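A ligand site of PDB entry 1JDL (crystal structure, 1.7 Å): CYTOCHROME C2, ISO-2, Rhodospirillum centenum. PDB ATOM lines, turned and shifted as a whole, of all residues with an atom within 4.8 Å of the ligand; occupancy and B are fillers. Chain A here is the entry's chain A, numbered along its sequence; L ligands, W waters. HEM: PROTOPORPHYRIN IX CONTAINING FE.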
ATOM      1  N   LYS A  14      16.798  15.868  -8.213  1.00  0.00           N
ATOM      2  CA  LYS A  14      16.453  14.803  -7.286  1.00  0.00           C
ATOM      3  C   LYS A  14      17.699  14.174  -6.660  1.00  0.00           C
ATOM      4  O   LYS A  14      17.589  13.358  -5.741  1.00  0.00           O
ATOM      5  CB  LYS A  14      15.654  13.709  -7.998  1.00  0.00           C
ATOM      6  CG  LYS A  14      14.300  14.174  -8.511  1.00  0.00           C
ATOM      7  CD  LYS A  14      13.564  13.025  -9.186  1.00  0.00           C
ATOM      8  CE  LYS A  14      12.185  13.464  -9.659  1.00  0.00           C
ATOM      9  NZ  LYS A  14      11.422  12.315 -10.222  1.00  0.00           N
ATOM     10  N   CYS A  15      18.873  14.549  -7.159  1.00  0.00           N
ATOM     11  CA  CYS A  15      20.134  14.006  -6.636  1.00  0.00           C
ATOM     12  C   CYS A  15      20.886  15.048  -5.834  1.00  0.00           C
ATOM     13  O   CYS A  15      21.703  14.706  -4.982  1.00  0.00           O
ATOM     14  CB  CYS A  15      21.074  13.581  -7.777  1.00  0.00           C
ATOM     15  SG  CYS A  15      20.349  12.753  -9.171  1.00  0.00           S
ATOM     16  N   CYS A  18      22.083  15.284  -2.024  1.00  0.00           N
ATOM     17  CA  CYS A  18      23.228  14.515  -1.560  1.00  0.00           C
ATOM     18  C   CYS A  18      24.456  14.486  -2.440  1.00  0.00           C
ATOM     19  O   CYS A  18      25.522  14.059  -2.001  1.00  0.00           O
ATOM     20  CB  CYS A  18      22.796  13.065  -1.318  1.00  0.00           C
ATOM     21  SG  CYS A  18      21.298  12.949  -0.361  1.00  0.00           S
ATOM     22  N   HIS A  19      24.315  14.923  -3.683  1.00  0.00           N
ATOM     23  CA  HIS A  19      25.436  14.897  -4.627  1.00  0.00           C
ATOM     24  C   HIS A  19      25.674  16.234  -5.297  1.00  0.00           C
ATOM     25  O   HIS A  19      24.759  17.045  -5.455  1.00  0.00           O
ATOM     26  CB  HIS A  19      25.170  13.894  -5.740  1.00  0.00           C
ATOM     27  CG  HIS A  19      25.168  12.465  -5.302  1.00  0.00           C
ATOM     28  ND1 HIS A  19      26.318  11.795  -4.958  1.00  0.00           N
ATOM     29  CD2 HIS A  19      24.161  11.578  -5.201  1.00  0.00           C
ATOM     30  CE1 HIS A  19      26.020  10.533  -4.692  1.00  0.00           C
ATOM     31  NE2 HIS A  19      24.713  10.379  -4.833  1.00  0.00           N
ATOM     32  N   VAL A  29      26.485  14.244   1.630  1.00  0.00           N
ATOM     33  CA  VAL A  29      26.039  12.981   2.200  1.00  0.00           C
ATOM     34  C   VAL A  29      26.500  11.873   1.255  1.00  0.00           C
ATOM     35  O   VAL A  29      26.810  10.759   1.679  1.00  0.00           O
ATOM     36  CB  VAL A  29      24.497  12.947   2.331  1.00  0.00           C
ATOM     37  CG1 VAL A  29      24.028  11.539   2.655  1.00  0.00           C
ATOM     38  CG2 VAL A  29      24.066  13.914   3.431  1.00  0.00           C
ATOM     39  N   GLY A  30      26.546  12.206  -0.038  1.00  0.00           N
ATOM     40  CA  GLY A  30      26.994  11.270  -1.051  1.00  0.00           C
ATOM     41  C   GLY A  30      28.264  11.793  -1.721  1.00  0.00           C
ATOM     42  O   GLY A  30      28.565  12.975  -1.619  1.00  0.00           O
ATOM     43  N   PRO A  31      29.010  10.945  -2.429  1.00  0.00           N
ATOM     44  CA  PRO A  31      30.238  11.386  -3.104  1.00  0.00           C
ATOM     45  C   PRO A  31      30.025  12.284  -4.308  1.00  0.00           C
ATOM     46  O   PRO A  31      28.982  12.228  -4.970  1.00  0.00           O
ATOM     47  CB  PRO A  31      30.922  10.063  -3.468  1.00  0.00           C
ATOM     48  CG  PRO A  31      29.761   9.147  -3.717  1.00  0.00           C
ATOM     49  CD  PRO A  31      28.821   9.482  -2.582  1.00  0.00           C
ATOM     50  N   LEU A  33      30.004  13.561  -7.966  1.00  0.00           N
ATOM     51  CA  LEU A  33      29.798  12.740  -9.148  1.00  0.00           C
ATOM     52  C   LEU A  33      30.517  13.226 -10.395  1.00  0.00           C
ATOM     53  O   LEU A  33      30.292  12.717 -11.493  1.00  0.00           O
ATOM     54  CB  LEU A  33      28.300  12.569  -9.419  1.00  0.00           C
ATOM     55  CG  LEU A  33      27.566  11.785  -8.319  1.00  0.00           C
ATOM     56  CD1 LEU A  33      26.076  11.748  -8.631  1.00  0.00           C
ATOM     57  CD2 LEU A  33      28.137  10.375  -8.217  1.00  0.00           C
ATOM     58  N   VAL A  36      32.416  10.534 -12.643  1.00  0.00           N
ATOM     59  CA  VAL A  36      31.962   9.222 -12.182  1.00  0.00           C
ATOM     60  C   VAL A  36      31.864   8.196 -13.312  1.00  0.00           C
ATOM     61  O   VAL A  36      31.976   6.991 -13.075  1.00  0.00           O
ATOM     62  CB  VAL A  36      30.604   9.339 -11.435  1.00  0.00           C
ATOM     63  CG1 VAL A  36      29.501   9.730 -12.414  1.00  0.00           C
ATOM     64  CG2 VAL A  36      30.279   8.023 -10.741  1.00  0.00           C
ATOM     65  N   ARG A  39      34.291   5.275 -13.689  1.00  0.00           N
ATOM     66  CA  ARG A  39      35.089   5.319 -12.465  1.00  0.00           C
ATOM     67  C   ARG A  39      34.790   4.058 -11.645  1.00  0.00           C
ATOM     68  O   ARG A  39      33.645   3.612 -11.589  1.00  0.00           O
ATOM     69  CB  ARG A  39      34.718   6.564 -11.646  1.00  0.00           C
ATOM     70  CG  ARG A  39      35.593   6.799 -10.402  1.00  0.00           C
ATOM     71  CD  ARG A  39      35.276   8.147  -9.741  1.00  0.00           C
ATOM     72  NE  ARG A  39      34.081   8.130  -8.909  1.00  0.00           N
ATOM     73  CZ  ARG A  39      33.414   9.217  -8.518  1.00  0.00           C
ATOM     74  NH1 ARG A  39      33.846  10.420  -8.904  1.00  0.00           N
ATOM     75  NH2 ARG A  39      32.346   9.121  -7.751  1.00  0.00           N
ATOM     76  N   ALA A  41      33.735   1.853  -8.710  1.00  0.00           N
ATOM     77  CA  ALA A  41      32.833   2.165  -7.605  1.00  0.00           C
ATOM     78  C   ALA A  41      33.600   2.262  -6.291  1.00  0.00           C
ATOM     79  O   ALA A  41      34.546   1.495  -6.060  1.00  0.00           O
ATOM     80  CB  ALA A  41      31.729   1.100  -7.498  1.00  0.00           C
ATOM     81  N   GLY A  42      33.203   3.202  -5.439  1.00  0.00           N
ATOM     82  CA  GLY A  42      33.826   3.361  -4.138  1.00  0.00           C
ATOM     83  C   GLY A  42      35.251   3.901  -4.093  1.00  0.00           C
ATOM     84  O   GLY A  42      36.015   3.523  -3.203  1.00  0.00           O
ATOM     85  N   THR A  43      35.592   4.792  -5.011  1.00  0.00           N
ATOM     86  CA  THR A  43      36.942   5.353  -5.028  1.00  0.00           C
ATOM     87  C   THR A  43      37.026   6.869  -5.025  1.00  0.00           C
ATOM     88  O   THR A  43      38.115   7.421  -5.185  1.00  0.00           O
ATOM     89  CB  THR A  43      37.754   4.841  -6.232  1.00  0.00           C
ATOM     90  OG1 THR A  43      37.099   5.245  -7.448  1.00  0.00           O
ATOM     91  CG2 THR A  43      37.880   3.329  -6.192  1.00  0.00           C
ATOM     92  N   ALA A  44      35.890   7.548  -4.862  1.00  0.00           N
ATOM     93  CA  ALA A  44      35.915   9.005  -4.838  1.00  0.00           C
ATOM     94  C   ALA A  44      36.764   9.422  -3.637  1.00  0.00           C
ATOM     95  O   ALA A  44      36.557   8.951  -2.520  1.00  0.00           O
ATOM     96  CB  ALA A  44      34.495   9.561  -4.700  1.00  0.00           C
ATOM     97  N   PHE A  47      35.774  10.179   0.507  1.00  0.00           N
ATOM     98  CA  PHE A  47      34.428   9.764   0.913  1.00  0.00           C
ATOM     99  C   PHE A  47      34.464   8.424   1.627  1.00  0.00           C
ATOM    100  O   PHE A  47      35.220   7.532   1.252  1.00  0.00           O
ATOM    101  CB  PHE A  47      33.512   9.662  -0.305  1.00  0.00           C
ATOM    102  CG  PHE A  47      32.079   9.390   0.066  1.00  0.00           C
ATOM    103  CD1 PHE A  47      31.265  10.422   0.524  1.00  0.00           C
ATOM    104  CD2 PHE A  47      31.577   8.096   0.018  1.00  0.00           C
ATOM    105  CE1 PHE A  47      29.954  10.169   0.932  1.00  0.00           C
ATOM    106  CE2 PHE A  47      30.270   7.830   0.426  1.00  0.00           C
ATOM    107  CZ  PHE A  47      29.457   8.862   0.884  1.00  0.00           C
ATOM    108  N   ASN A  48      33.636   8.293   2.670  1.00  0.00           N
ATOM    109  CA  ASN A  48      33.578   7.046   3.418  1.00  0.00           C
ATOM    110  C   ASN A  48      32.391   6.206   2.974  1.00  0.00           C
ATOM    111  O   ASN A  48      31.247   6.433   3.381  1.00  0.00           O
ATOM    112  CB  ASN A  48      33.517   7.312   4.925  1.00  0.00           C
ATOM    113  CG  ASN A  48      34.847   7.776   5.481  1.00  0.00           C
ATOM    114  OD1 ASN A  48      35.892   7.209   5.161  1.00  0.00           O
ATOM    115  ND2 ASN A  48      34.812   8.808   6.316  1.00  0.00           N
ATOM    116  N   TYR A  49      32.690   5.231   2.121  1.00  0.00           N
ATOM    117  CA  TYR A  49      31.722   4.326   1.544  1.00  0.00           C
ATOM    118  C   TYR A  49      31.282   3.190   2.460  1.00  0.00           C
ATOM    119  O   TYR A  49      31.958   2.866   3.437  1.00  0.00           O
ATOM    120  CB  TYR A  49      32.311   3.692   0.286  1.00  0.00           C
ATOM    121  CG  TYR A  49      32.456   4.639  -0.868  1.00  0.00           C
ATOM    122  CD1 TYR A  49      31.395   4.874  -1.748  1.00  0.00           C
ATOM    123  CD2 TYR A  49      33.663   5.290  -1.110  1.00  0.00           C
ATOM    124  CE1 TYR A  49      31.535   5.733  -2.845  1.00  0.00           C
ATOM    125  CE2 TYR A  49      33.815   6.145  -2.199  1.00  0.00           C
ATOM    126  CZ  TYR A  49      32.761   6.359  -3.059  1.00  0.00           C
ATOM    127  OH  TYR A  49      32.934   7.147  -4.161  1.00  0.00           O
ATOM    128  N   SER A  50      30.150   2.589   2.124  1.00  0.00           N
ATOM    129  CA  SER A  50      29.644   1.439   2.863  1.00  0.00           C
ATOM    130  C   SER A  50      30.544   0.286   2.438  1.00  0.00           C
ATOM    131  O   SER A  50      31.221   0.363   1.401  1.00  0.00           O
ATOM    132  CB  SER A  50      28.210   1.126   2.454  1.00  0.00           C
ATOM    133  OG  SER A  50      28.156   0.759   1.091  1.00  0.00           O
ATOM    134  N   ASN A  53      29.436  -0.998  -1.126  1.00  0.00           N
ATOM    135  CA  ASN A  53      29.774  -0.170  -2.280  1.00  0.00           C
ATOM    136  C   ASN A  53      31.283  -0.313  -2.549  1.00  0.00           C
ATOM    137  O   ASN A  53      31.709  -0.409  -3.691  1.00  0.00           O
ATOM    138  CB  ASN A  53      29.429   1.299  -1.992  1.00  0.00           C
ATOM    139  CG  ASN A  53      29.457   2.172  -3.234  1.00  0.00           C
ATOM    140  OD1 ASN A  53      30.370   2.073  -4.050  1.00  0.00           O
ATOM    141  ND2 ASN A  53      28.471   3.039  -3.374  1.00  0.00           N
ATOM    142  N   TRP A  63      31.466   2.447 -13.082  1.00  0.00           N
ATOM    143  CA  TRP A  63      30.209   3.073 -13.444  1.00  0.00           C
ATOM    144  C   TRP A  63      30.029   3.455 -14.902  1.00  0.00           C
ATOM    145  O   TRP A  63      30.034   4.640 -15.266  1.00  0.00           O
ATOM    146  CB  TRP A  63      29.962   4.297 -12.557  1.00  0.00           C
ATOM    147  CG  TRP A  63      29.697   3.909 -11.124  1.00  0.00           C
ATOM    148  CD1 TRP A  63      30.427   4.260 -10.030  1.00  0.00           C
ATOM    149  CD2 TRP A  63      28.646   3.054 -10.647  1.00  0.00           C
ATOM    150  NE1 TRP A  63      29.904   3.676  -8.898  1.00  0.00           N
ATOM    151  CE2 TRP A  63      28.804   2.937  -9.247  1.00  0.00           C
ATOM    152  CE3 TRP A  63      27.585   2.381 -11.272  1.00  0.00           C
ATOM    153  CZ2 TRP A  63      27.947   2.164  -8.456  1.00  0.00           C
ATOM    154  CZ3 TRP A  63      26.716   1.611 -10.487  1.00  0.00           C
ATOM    155  CH2 TRP A  63      26.906   1.513  -9.088  1.00  0.00           C
ATOM    156  N   ILE A  68      25.038   2.407 -14.438  1.00  0.00           N
ATOM    157  CA  ILE A  68      24.349   3.412 -13.640  1.00  0.00           C
ATOM    158  C   ILE A  68      22.846   3.291 -13.892  1.00  0.00           C
ATOM    159  O   ILE A  68      22.034   3.375 -12.969  1.00  0.00           O
ATOM    160  CB  ILE A  68      24.821   4.837 -13.986  1.00  0.00           C
ATOM    161  CG1 ILE A  68      26.330   4.953 -13.746  1.00  0.00           C
ATOM    162  CG2 ILE A  68      24.071   5.856 -13.139  1.00  0.00           C
ATOM    163  CD1 ILE A  68      26.914   6.319 -14.080  1.00  0.00           C
ATOM    164  N   TYR A  71      21.492   0.386 -12.064  1.00  0.00           N
ATOM    165  CA  TYR A  71      21.669   0.590 -10.624  1.00  0.00           C
ATOM    166  C   TYR A  71      20.602   1.469  -9.979  1.00  0.00           C
ATOM    167  O   TYR A  71      20.071   1.143  -8.920  1.00  0.00           O
ATOM    168  CB  TYR A  71      23.055   1.212 -10.405  1.00  0.00           C
ATOM    169  CG  TYR A  71      23.313   1.893  -9.075  1.00  0.00           C
ATOM    170  CD1 TYR A  71      23.623   1.153  -7.928  1.00  0.00           C
ATOM    171  CD2 TYR A  71      23.322   3.281  -8.981  1.00  0.00           C
ATOM    172  CE1 TYR A  71      23.949   1.790  -6.731  1.00  0.00           C
ATOM    173  CE2 TYR A  71      23.641   3.931  -7.792  1.00  0.00           C
ATOM    174  CZ  TYR A  71      23.960   3.181  -6.680  1.00  0.00           C
ATOM    175  OH  TYR A  71      24.315   3.822  -5.512  1.00  0.00           O
ATOM    176  N   LEU A  72      20.299   2.598 -10.615  1.00  0.00           N
ATOM    177  CA  LEU A  72      19.353   3.571 -10.074  1.00  0.00           C
ATOM    178  C   LEU A  72      17.961   3.135  -9.591  1.00  0.00           C
ATOM    179  O   LEU A  72      17.448   3.691  -8.634  1.00  0.00           O
ATOM    180  CB  LEU A  72      19.213   4.745 -11.041  1.00  0.00           C
ATOM    181  CG  LEU A  72      20.457   5.640 -11.128  1.00  0.00           C
ATOM    182  CD1 LEU A  72      20.256   6.701 -12.198  1.00  0.00           C
ATOM    183  CD2 LEU A  72      20.745   6.279  -9.774  1.00  0.00           C
ATOM    184  N   THR A  96      23.724  -0.554   1.091  1.00  0.00           N
ATOM    185  CA  THR A  96      24.339   0.706   0.680  1.00  0.00           C
ATOM    186  C   THR A  96      23.739   1.888   1.443  1.00  0.00           C
ATOM    187  O   THR A  96      22.578   1.837   1.870  1.00  0.00           O
ATOM    188  CB  THR A  96      24.160   0.965  -0.846  1.00  0.00           C
ATOM    189  OG1 THR A  96      24.736   2.232  -1.194  1.00  0.00           O
ATOM    190  CG2 THR A  96      22.686   0.988  -1.207  1.00  0.00           C
ATOM    191  N   LYS A  97      24.522   2.945   1.609  1.00  0.00           N
ATOM    192  CA  LYS A  97      24.086   4.142   2.313  1.00  0.00           C
ATOM    193  C   LYS A  97      23.151   4.991   1.459  1.00  0.00           C
ATOM    194  O   LYS A  97      22.523   5.928   1.971  1.00  0.00           O
ATOM    195  CB  LYS A  97      25.281   4.994   2.722  1.00  0.00           C
ATOM    196  CG  LYS A  97      26.179   4.377   3.784  1.00  0.00           C
ATOM    197  CD  LYS A  97      27.327   5.314   4.119  1.00  0.00           C
ATOM    198  CE  LYS A  97      28.261   4.710   5.159  1.00  0.00           C
ATOM    199  NZ  LYS A  97      29.342   5.651   5.535  1.00  0.00           N
ATOM    200  N   MET A  98      23.060   4.697   0.165  1.00  0.00           N
ATOM    201  CA  MET A  98      22.175   5.467  -0.699  1.00  0.00           C
ATOM    202  C   MET A  98      20.750   4.959  -0.631  1.00  0.00           C
ATOM    203  O   MET A  98      20.413   3.933  -1.242  1.00  0.00           O
ATOM    204  CB  MET A  98      22.645   5.426  -2.160  1.00  0.00           C
ATOM    205  CG  MET A  98      21.761   6.273  -3.081  1.00  0.00           C
ATOM    206  SD  MET A  98      22.504   6.570  -4.702  1.00  0.00           S
ATOM    207  CE  MET A  98      21.075   6.451  -5.748  1.00  0.00           C
ATOM    208  N   VAL A  99      19.935   5.672   0.146  1.00  0.00           N
ATOM    209  CA  VAL A  99      18.537   5.340   0.333  1.00  0.00           C
ATOM    210  C   VAL A  99      17.681   6.234  -0.567  1.00  0.00           C
ATOM    211  O   VAL A  99      17.026   7.164  -0.098  1.00  0.00           O
ATOM    212  CB  VAL A  99      18.104   5.544   1.806  1.00  0.00           C
ATOM    213  CG1 VAL A  99      16.669   5.086   2.000  1.00  0.00           C
ATOM    214  CG2 VAL A  99      19.037   4.788   2.739  1.00  0.00           C
ATOM    215  N   PHE A 100      17.745   5.950  -1.855  1.00  0.00           N
ATOM    216  CA  PHE A 100      16.983   6.695  -2.858  1.00  0.00           C
ATOM    217  C   PHE A 100      16.920   5.831  -4.111  1.00  0.00           C
ATOM    218  O   PHE A 100      17.876   5.136  -4.440  1.00  0.00           O
ATOM    219  CB  PHE A 100      17.684   8.035  -3.173  1.00  0.00           C
ATOM    220  CG  PHE A 100      16.933   8.888  -4.165  1.00  0.00           C
ATOM    221  CD1 PHE A 100      17.178   8.777  -5.525  1.00  0.00           C
ATOM    222  CD2 PHE A 100      15.967   9.784  -3.728  1.00  0.00           C
ATOM    223  CE1 PHE A 100      16.466   9.536  -6.450  1.00  0.00           C
ATOM    224  CE2 PHE A 100      15.245  10.561  -4.641  1.00  0.00           C
ATOM    225  CZ  PHE A 100      15.503  10.433  -6.004  1.00  0.00           C
ATOM    226  N   LEU A 102      15.341   5.692  -8.325  1.00  0.00           N
ATOM    227  CA  LEU A 102      14.838   6.440  -9.478  1.00  0.00           C
ATOM    228  C   LEU A 102      14.364   5.346 -10.431  1.00  0.00           C
ATOM    229  O   LEU A 102      15.122   4.879 -11.277  1.00  0.00           O
ATOM    230  CB  LEU A 102      15.962   7.255 -10.120  1.00  0.00           C
ATOM    231  CG  LEU A 102      15.574   8.301 -11.176  1.00  0.00           C
ATOM    232  CD1 LEU A 102      16.843   8.837 -11.836  1.00  0.00           C
ATOM    233  CD2 LEU A 102      14.685   7.682 -12.240  1.00  0.00           C
ATOM    234  N   VAL A 111      19.268  11.523 -16.784  1.00  0.00           N
ATOM    235  CA  VAL A 111      20.211  11.944 -15.757  1.00  0.00           C
ATOM    236  C   VAL A 111      21.602  11.410 -16.086  1.00  0.00           C
ATOM    237  O   VAL A 111      22.606  12.067 -15.819  1.00  0.00           O
ATOM    238  CB  VAL A 111      19.740  11.499 -14.344  1.00  0.00           C
ATOM    239  CG1 VAL A 111      19.981  10.011 -14.131  1.00  0.00           C
ATOM    240  CG2 VAL A 111      20.461  12.336 -13.283  1.00  0.00           C
ATOM    241  N   LEU A 115      25.121  13.351 -16.581  1.00  0.00           N
ATOM    242  CA  LEU A 115      26.357  12.993 -15.892  1.00  0.00           C
ATOM    243  C   LEU A 115      27.512  12.793 -16.858  1.00  0.00           C
ATOM    244  O   LEU A 115      28.667  13.032 -16.500  1.00  0.00           O
ATOM    245  CB  LEU A 115      26.151  11.727 -15.059  1.00  0.00           C
ATOM    246  CG  LEU A 115      25.255  11.870 -13.833  1.00  0.00           C
ATOM    247  CD1 LEU A 115      25.015  10.504 -13.203  1.00  0.00           C
ATOM    248  CD2 LEU A 115      25.891  12.831 -12.847  1.00  0.00           C
HETATM  249  CHA HEM L   1      26.305   6.737  -4.136  1.00  0.00           C
HETATM  250  CHB HEM L   1      24.122   8.303  -8.134  1.00  0.00           C
HETATM  251  CHC HEM L   1      20.708  10.397  -5.432  1.00  0.00           C
HETATM  252  CHD HEM L   1      23.189   9.300  -1.483  1.00  0.00           C
HETATM  253  C1A HEM L   1      25.975   6.939  -5.479  1.00  0.00           C
HETATM  254  C2A HEM L   1      26.674   6.329  -6.581  1.00  0.00           C
HETATM  255  C3A HEM L   1      26.042   6.774  -7.702  1.00  0.00           C
HETATM  256  C4A HEM L   1      24.983   7.653  -7.279  1.00  0.00           C
HETATM  257  CMA HEM L   1      26.342   6.379  -9.147  1.00  0.00           C
HETATM  258  CAA HEM L   1      27.956   5.501  -6.478  1.00  0.00           C
HETATM  259  CBA HEM L   1      29.129   6.476  -6.548  1.00  0.00           C
HETATM  260  CGA HEM L   1      30.505   5.825  -6.335  1.00  0.00           C
HETATM  261  O1A HEM L   1      30.591   4.596  -6.235  1.00  0.00           O
HETATM  262  O2A HEM L   1      31.503   6.580  -6.269  1.00  0.00           O
HETATM  263  C1B HEM L   1      23.018   9.032  -7.732  1.00  0.00           C
HETATM  264  C2B HEM L   1      22.078   9.664  -8.635  1.00  0.00           C
HETATM  265  C3B HEM L   1      21.018  10.043  -7.853  1.00  0.00           C
HETATM  266  C4B HEM L   1      21.425   9.883  -6.514  1.00  0.00           C
HETATM  267  CMB HEM L   1      22.292   9.864 -10.128  1.00  0.00           C
HETATM  268  CAB HEM L   1      19.662  10.242  -8.185  1.00  0.00           C
HETATM  269  CBB HEM L   1      18.981  10.057  -9.531  1.00  0.00           C
HETATM  270  C1C HEM L   1      21.062  10.243  -4.130  1.00  0.00           C
HETATM  271  C2C HEM L   1      20.317  10.767  -2.999  1.00  0.00           C
HETATM  272  C3C HEM L   1      20.933  10.304  -1.904  1.00  0.00           C
HETATM  273  C4C HEM L   1      22.189   9.721  -2.348  1.00  0.00           C
HETATM  274  CMC HEM L   1      19.085  11.679  -3.070  1.00  0.00           C
HETATM  275  CAC HEM L   1      20.462  10.187  -0.581  1.00  0.00           C
HETATM  276  CBC HEM L   1      19.181  10.728   0.060  1.00  0.00           C
HETATM  277  C1D HEM L   1      24.301   8.572  -1.856  1.00  0.00           C
HETATM  278  C2D HEM L   1      25.235   8.004  -0.922  1.00  0.00           C
HETATM  279  C3D HEM L   1      26.080   7.208  -1.652  1.00  0.00           C
HETATM  280  C4D HEM L   1      25.653   7.334  -3.046  1.00  0.00           C
HETATM  281  CMD HEM L   1      25.250   8.184   0.598  1.00  0.00           C
HETATM  282  CAD HEM L   1      27.181   6.299  -1.094  1.00  0.00           C
HETATM  283  CBD HEM L   1      26.532   4.916  -0.886  1.00  0.00           C
HETATM  284  CGD HEM L   1      27.441   3.917  -0.195  1.00  0.00           C
HETATM  285  O1D HEM L   1      26.969   2.783   0.043  1.00  0.00           O
HETATM  286  O2D HEM L   1      28.610   4.248   0.092  1.00  0.00           O
HETATM  287  NA  HEM L   1      24.931   7.726  -5.900  1.00  0.00           N
HETATM  288  NB  HEM L   1      22.618   9.181  -6.422  1.00  0.00           N
HETATM  289  NC  HEM L   1      22.201   9.580  -3.711  1.00  0.00           N
HETATM  290  ND  HEM L   1      24.545   8.172  -3.159  1.00  0.00           N
HETATM  291 FE   HEM L   1      23.545   8.641  -4.799  1.00  0.00          FE
HETATM  292  O   HOH W   1      26.729   8.873   3.687  1.00  0.00           O
HETATM  293  O   HOH W   2      21.464   8.352   1.607  1.00  0.00           O
HETATM  294  O   HOH W   3      33.763   5.903  -7.284  1.00  0.00           O
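O1D of the ligand lies within hydrogen-bond range of OG of Ser 50, at 2.6 Å. An iron atom (FE) of the ligand is bound by a ring nitrogen (NE2) of His 19 (2.1 Å). NH2 of Arg 39 lies within salt-bridge range of O2A of the ligand (3.1 Å). O1A of the ligand lies close to OD1 of Asn 53 (3.3 Å). N of Lys 97 is in hydrogen-bond range of O1D of the ligand (2.9 Å). SD of Met 98 binds FE of the ligand, at 2.3 Å. The side-chain hydroxyl (OH) of Tyr 49 is in hydrogen-bond range of an oxygen (O2A) of the ligand. The backbone NH (N) of Ser 50 sits at hydrogen-bond distance from an oxygen (O2D) of the ligand (3.0 Å). The side-chain hydroxyl (OG1) of Thr 96 sits at hydrogen-bond distance from an oxygen (O1D) of the ligand (2.6 Å). N of Gly 42 lies within hydrogen-bond range of O1A of the ligand (3.1 Å). O1A of the ligand lies within hydrogen-bond range of NE1 of Trp 63.
N of Leu 102 sits at hydrogen-bond distance from O of Leu 72 (2.9 Å). The side-chain hydroxyl of Tyr 49 sits close to the backbone NH of Ala 44 (3.1 Å). The backbone NH of Trp 63 sits at hydrogen-bond distance from the backbone carbonyl oxygen of Arg 39 (2.9 Å). The side-chain amide oxygen of Asn 53 sits at hydrogen-bond distance from the backbone NH of Gly 42 (3.4 Å). SD of Met 98 sits close to OH of Tyr 71. The side-chain amino group (NZ) of Lys 97 sits at hydrogen-bond distance from the backbone carbonyl oxygen (O) of Asn 48 (3.0 Å). N of Met 98 lies close to OG1 of Thr 96, at 3.3 Å. The backbone carbonyl oxygen (O) of Cys 18 sits at hydrogen-bond distance from the backbone NH (N) of Gly 30 (2.9 Å).
Lys 14 touches the ligand. Cys 15 touches the ligand. Cys 18 touches the ligand. Val 29 touches the ligand. Gly 30 touches the ligand (CA to C2D, 3.7 Å). Pro 31 touches the ligand (CD to C3D, 3.7 Å). CD1 of Leu 33 touches CHB of the ligand, 3.99 Å away. CA of Ala 41 touches O1A of the ligand, at 3.6 Å. Phe 47 touches the ligand (CE2 to CAD, 3.8 Å). Tyr 71 touches the ligand (OH to C1A, 3.5 Å). CD2 of Leu 72 touches C2B of the ligand, at 3.8 Å. Phe 100 touches the ligand (CG to CMC, 3.7 Å). CD1 of Leu 102 touches CBB of the ligand (3.4 Å). 23 residues have an atom within 4 Å of the ligand: Lys 14, Cys 15, Cys 18, His 19, Val 29, Gly 30, Pro 31, Leu 33, Arg 39, Ala 41, Gly 42, Phe 47, Tyr 49, Ser 50, Asn 53, Trp 63, Tyr 71, Leu 72, Thr 96, Lys 97, Met 98, Phe 100 and Leu 102. The nearest printed residue that does not touch the ligand is Leu 115 (4.2 Å).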
